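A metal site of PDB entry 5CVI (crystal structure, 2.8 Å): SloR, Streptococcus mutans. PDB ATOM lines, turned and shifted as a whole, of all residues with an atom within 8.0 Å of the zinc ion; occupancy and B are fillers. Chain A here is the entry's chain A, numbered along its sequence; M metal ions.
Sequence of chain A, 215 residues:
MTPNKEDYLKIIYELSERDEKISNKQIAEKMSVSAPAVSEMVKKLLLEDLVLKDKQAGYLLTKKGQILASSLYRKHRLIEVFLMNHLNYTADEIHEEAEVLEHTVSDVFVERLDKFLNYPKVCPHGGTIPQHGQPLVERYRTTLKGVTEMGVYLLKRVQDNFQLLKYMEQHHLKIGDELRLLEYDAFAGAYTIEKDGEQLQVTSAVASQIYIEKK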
ATOM      1  N   PRO A   3     -12.831  13.031  14.851  1.00  0.00           N
ATOM      2  CA  PRO A   3     -13.920  12.228  15.422  1.00  0.00           C
ATOM      3  C   PRO A   3     -15.097  13.098  15.844  1.00  0.00           C
ATOM      4  O   PRO A   3     -14.994  13.810  16.848  1.00  0.00           O
ATOM      5  CB  PRO A   3     -13.278  11.590  16.656  1.00  0.00           C
ATOM      6  CG  PRO A   3     -11.820  11.609  16.389  1.00  0.00           C
ATOM      7  CD  PRO A   3     -11.571  12.861  15.596  1.00  0.00           C
ATOM      8  N   ASN A   4     -16.200  13.041  15.105  1.00  0.00           N
ATOM      9  CA  ASN A   4     -17.377  13.849  15.419  1.00  0.00           C
ATOM     10  C   ASN A   4     -18.073  13.382  16.700  1.00  0.00           C
ATOM     11  O   ASN A   4     -17.642  12.413  17.332  1.00  0.00           O
ATOM     12  CB  ASN A   4     -18.359  13.853  14.250  1.00  0.00           C
ATOM     13  CG  ASN A   4     -18.871  12.469  13.917  1.00  0.00           C
ATOM     14  OD1 ASN A   4     -18.201  11.463  14.148  1.00  0.00           O
ATOM     15  ND2 ASN A   4     -20.082  12.406  13.353  1.00  0.00           N
ATOM     16  N   LYS A   5     -19.130  14.082  17.083  1.00  0.00           N
ATOM     17  CA  LYS A   5     -19.849  13.774  18.322  1.00  0.00           C
ATOM     18  C   LYS A   5     -20.388  12.353  18.354  1.00  0.00           C
ATOM     19  O   LYS A   5     -20.425  11.717  19.398  1.00  0.00           O
ATOM     20  CB  LYS A   5     -20.993  14.775  18.549  1.00  0.00           C
ATOM     21  CG  LYS A   5     -22.051  14.761  17.469  1.00  0.00           C
ATOM     22  CD  LYS A   5     -23.263  15.594  17.843  1.00  0.00           C
ATOM     23  CE  LYS A   5     -24.308  15.552  16.736  1.00  0.00           C
ATOM     24  NZ  LYS A   5     -25.521  16.337  17.064  1.00  0.00           N
ATOM     25  N   GLU A   6     -20.802  11.856  17.184  1.00  0.00           N
ATOM     26  CA  GLU A   6     -21.384  10.523  17.084  1.00  0.00           C
ATOM     27  C   GLU A   6     -20.390   9.440  17.481  1.00  0.00           C
ATOM     28  O   GLU A   6     -20.781   8.360  17.936  1.00  0.00           O
ATOM     29  CB  GLU A   6     -21.917  10.291  15.666  1.00  0.00           C
ATOM     30  CG  GLU A   6     -23.018  11.259  15.267  1.00  0.00           C
ATOM     31  CD  GLU A   6     -23.152  11.416  13.767  1.00  0.00           C
ATOM     32  OE1 GLU A   6     -22.414  12.247  13.188  1.00  0.00           O
ATOM     33  OE2 GLU A   6     -24.001  10.723  13.169  1.00  0.00           O
ATOM     34  N   ASP A   7     -19.102   9.725  17.307  1.00  0.00           N
ATOM     35  CA  ASP A   7     -18.055   8.790  17.694  1.00  0.00           C
ATOM     36  C   ASP A   7     -18.002   8.618  19.205  1.00  0.00           C
ATOM     37  O   ASP A   7     -17.731   7.528  19.714  1.00  0.00           O
ATOM     38  CB  ASP A   7     -16.706   9.255  17.165  1.00  0.00           C
ATOM     39  CG  ASP A   7     -16.489   8.878  15.714  1.00  0.00           C
ATOM     40  OD1 ASP A   7     -17.103   7.886  15.271  1.00  0.00           O
ATOM     41  OD2 ASP A   7     -15.711   9.567  15.027  1.00  0.00           O
ATOM     42  N   TYR A   8     -18.269   9.708  19.917  1.00  0.00           N
ATOM     43  CA  TYR A   8     -18.265   9.712  21.376  1.00  0.00           C
ATOM     44  C   TYR A   8     -19.375   8.822  21.938  1.00  0.00           C
ATOM     45  O   TYR A   8     -19.220   8.238  23.012  1.00  0.00           O
ATOM     46  CB  TYR A   8     -18.396  11.147  21.887  1.00  0.00           C
ATOM     47  CG  TYR A   8     -17.144  11.976  21.683  1.00  0.00           C
ATOM     48  CD1 TYR A   8     -16.301  12.259  22.749  1.00  0.00           C
ATOM     49  CD2 TYR A   8     -16.793  12.445  20.424  1.00  0.00           C
ATOM     50  CE1 TYR A   8     -15.147  13.000  22.567  1.00  0.00           C
ATOM     51  CE2 TYR A   8     -15.640  13.191  20.234  1.00  0.00           C
ATOM     52  CZ  TYR A   8     -14.828  13.467  21.311  1.00  0.00           C
ATOM     53  OH  TYR A   8     -13.686  14.213  21.133  1.00  0.00           O
ATOM     54  N   LYS A  10     -20.478   5.957  20.604  1.00  0.00           N
ATOM     55  CA  LYS A  10     -20.009   4.581  20.514  1.00  0.00           C
ATOM     56  C   LYS A  10     -19.023   4.259  21.625  1.00  0.00           C
ATOM     57  O   LYS A  10     -18.942   3.117  22.083  1.00  0.00           O
ATOM     58  CB  LYS A  10     -19.377   4.309  19.142  1.00  0.00           C
ATOM     59  CG  LYS A  10     -20.351   4.436  17.977  1.00  0.00           C
ATOM     60  CD  LYS A  10     -19.771   3.878  16.692  1.00  0.00           C
ATOM     61  CE  LYS A  10     -18.488   4.609  16.291  1.00  0.00           C
ATOM     62  NZ  LYS A  10     -17.817   3.947  15.136  1.00  0.00           N
ATOM     63  N   LEU A  72     -25.324   3.610  13.896  1.00  0.00           N
ATOM     64  CA  LEU A  72     -23.900   3.731  13.593  1.00  0.00           C
ATOM     65  C   LEU A  72     -23.223   2.369  13.502  1.00  0.00           C
ATOM     66  O   LEU A  72     -22.465   2.120  12.565  1.00  0.00           O
ATOM     67  CB  LEU A  72     -23.186   4.604  14.628  1.00  0.00           C
ATOM     68  CG  LEU A  72     -22.914   6.056  14.223  1.00  0.00           C
ATOM     69  CD1 LEU A  72     -21.444   6.399  14.419  1.00  0.00           C
ATOM     70  CD2 LEU A  72     -23.335   6.284  12.775  1.00  0.00           C
ATOM     71  N   HIS A  76     -21.443   0.746  10.216  1.00  0.00           N
ATOM     72  CA  HIS A  76     -20.053   0.327  10.377  1.00  0.00           C
ATOM     73  C   HIS A  76     -19.861  -1.142  10.045  1.00  0.00           C
ATOM     74  O   HIS A  76     -18.941  -1.502   9.306  1.00  0.00           O
ATOM     75  CB  HIS A  76     -19.602   0.600  11.813  1.00  0.00           C
ATOM     76  CG  HIS A  76     -18.112   0.579  11.983  1.00  0.00           C
ATOM     77  ND1 HIS A  76     -17.319   1.664  11.670  1.00  0.00           N
ATOM     78  CD2 HIS A  76     -17.278  -0.376  12.447  1.00  0.00           C
ATOM     79  CE1 HIS A  76     -16.054   1.361  11.923  1.00  0.00           C
ATOM     80  NE2 HIS A  76     -16.009   0.136  12.398  1.00  0.00           N
ATOM     81  N   HIS A  95     -10.955  -0.553   9.683  1.00  0.00           N
ATOM     82  CA  HIS A  95     -11.556   0.410  10.599  1.00  0.00           C
ATOM     83  C   HIS A  95     -11.654   1.826  10.045  1.00  0.00           C
ATOM     84  O   HIS A  95     -12.754   2.375   9.931  1.00  0.00           O
ATOM     85  CB  HIS A  95     -10.859   0.440  11.958  1.00  0.00           C
ATOM     86  CG  HIS A  95     -11.513   1.360  12.937  1.00  0.00           C
ATOM     87  ND1 HIS A  95     -12.770   1.115  13.442  1.00  0.00           N
ATOM     88  CD2 HIS A  95     -11.100   2.527  13.486  1.00  0.00           C
ATOM     89  CE1 HIS A  95     -13.111   2.092  14.262  1.00  0.00           C
ATOM     90  NE2 HIS A  95     -12.109   2.959  14.314  1.00  0.00           N
ATOM     91  N   ALA A  98     -14.042   2.040   7.157  1.00  0.00           N
ATOM     92  CA  ALA A  98     -15.427   1.896   7.601  1.00  0.00           C
ATOM     93  C   ALA A  98     -15.849   3.086   8.456  1.00  0.00           C
ATOM     94  O   ALA A  98     -17.012   3.446   8.513  1.00  0.00           O
ATOM     95  CB  ALA A  98     -15.604   0.599   8.376  1.00  0.00           C
ATOM     96  N   GLU A  99     -14.871   3.674   9.123  1.00  0.00           N
ATOM     97  CA  GLU A  99     -15.097   4.822   9.983  1.00  0.00           C
ATOM     98  C   GLU A  99     -15.498   6.045   9.172  1.00  0.00           C
ATOM     99  O   GLU A  99     -16.433   6.761   9.550  1.00  0.00           O
ATOM    100  CB  GLU A  99     -13.824   5.124  10.804  1.00  0.00           C
ATOM    101  CG  GLU A  99     -13.940   6.307  11.727  1.00  0.00           C
ATOM    102  CD  GLU A  99     -15.173   6.234  12.606  1.00  0.00           C
ATOM    103  OE1 GLU A  99     -15.541   5.105  13.012  1.00  0.00           O
ATOM    104  OE2 GLU A  99     -15.775   7.291  12.875  1.00  0.00           O
ATOM    105  N   VAL A 100     -14.804   6.269   8.072  1.00  0.00           N
ATOM    106  CA  VAL A 100     -15.108   7.389   7.189  1.00  0.00           C
ATOM    107  C   VAL A 100     -16.460   7.216   6.496  1.00  0.00           C
ATOM    108  O   VAL A 100     -17.269   8.153   6.445  1.00  0.00           O
ATOM    109  CB  VAL A 100     -13.993   7.594   6.130  1.00  0.00           C
ATOM    110  CG1 VAL A 100     -14.545   8.223   4.870  1.00  0.00           C
ATOM    111  CG2 VAL A 100     -12.866   8.437   6.707  1.00  0.00           C
ATOM    112  N   LEU A 101     -16.703   6.016   5.981  1.00  0.00           N
ATOM    113  CA  LEU A 101     -17.913   5.728   5.228  1.00  0.00           C
ATOM    114  C   LEU A 101     -19.204   5.800   6.039  1.00  0.00           C
ATOM    115  O   LEU A 101     -20.254   6.191   5.517  1.00  0.00           O
ATOM    116  CB  LEU A 101     -17.810   4.350   4.546  1.00  0.00           C
ATOM    117  CG  LEU A 101     -16.819   4.244   3.388  1.00  0.00           C
ATOM    118  CD1 LEU A 101     -16.846   2.851   2.790  1.00  0.00           C
ATOM    119  CD2 LEU A 101     -17.154   5.285   2.335  1.00  0.00           C
ATOM    120  N   GLU A 102     -19.141   5.422   7.313  1.00  0.00           N
ATOM    121  CA  GLU A 102     -20.332   5.416   8.165  1.00  0.00           C
ATOM    122  C   GLU A 102     -20.854   6.849   8.378  1.00  0.00           C
ATOM    123  O   GLU A 102     -22.010   7.036   8.740  1.00  0.00           O
ATOM    124  CB  GLU A 102     -20.052   4.750   9.511  1.00  0.00           C
ATOM    125  CG  GLU A 102     -19.280   5.625  10.497  1.00  0.00           C
ATOM    126  CD  GLU A 102     -19.118   4.983  11.866  1.00  0.00           C
ATOM    127  OE1 GLU A 102     -19.404   3.778  12.002  1.00  0.00           O
ATOM    128  OE2 GLU A 102     -18.711   5.701  12.798  1.00  0.00           O
ATOM    129  N   HIS A 103     -19.998   7.834   8.144  1.00  0.00           N
ATOM    130  CA  HIS A 103     -20.385   9.231   8.302  1.00  0.00           C
ATOM    131  C   HIS A 103     -20.672   9.913   6.966  1.00  0.00           C
ATOM    132  O   HIS A 103     -20.975  11.102   6.924  1.00  0.00           O
ATOM    133  CB  HIS A 103     -19.297   9.997   9.058  1.00  0.00           C
ATOM    134  CG  HIS A 103     -19.126   9.554  10.469  1.00  0.00           C
ATOM    135  ND1 HIS A 103     -20.124   9.643  11.405  1.00  0.00           N
ATOM    136  CD2 HIS A 103     -18.062   9.011  11.104  1.00  0.00           C
ATOM    137  CE1 HIS A 103     -19.688   9.177  12.566  1.00  0.00           C
ATOM    138  NE2 HIS A 103     -18.432   8.788  12.408  1.00  0.00           N
HETATM  139 ZN    ZN M   1     -17.633   7.245  13.447  1.00  0.00          ZN
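The side-chain carboxylate (OE1) of Glu 99 is in salt-bridge range of the side-chain amino group (NZ) of Lys 10 (3.3 Å). ND1 of His 103 sits close to ND2 of Asn 4, 3.4 Å away. A ring nitrogen (ND1) of His 76 sits at hydrogen-bond distance from the side-chain carboxylate (OE1) of Glu 102, 3.0 Å away. The side-chain carboxylate (OD2) of Asp 7 sits close to the side-chain amide oxygen (OD1) of Asn 4 (3.3 Å). OE1 of Glu 102 lies within salt-bridge range of NZ of Lys 10, 3.5 Å away.
The zinc ion is bound by OE2 of Glu 99 (1.9 Å), OE2 of Glu 102 (2.0 Å), OD1 of Asp 7 (2.0 Å) and NE2 of His 103 (2.0 Å).
NZ of Lys 10 touches the zinc ion, 3.7 Å away. Within 4 Å of the zinc ion: Asp 7, Lys 10, Glu 99, Glu 102 and His 103.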
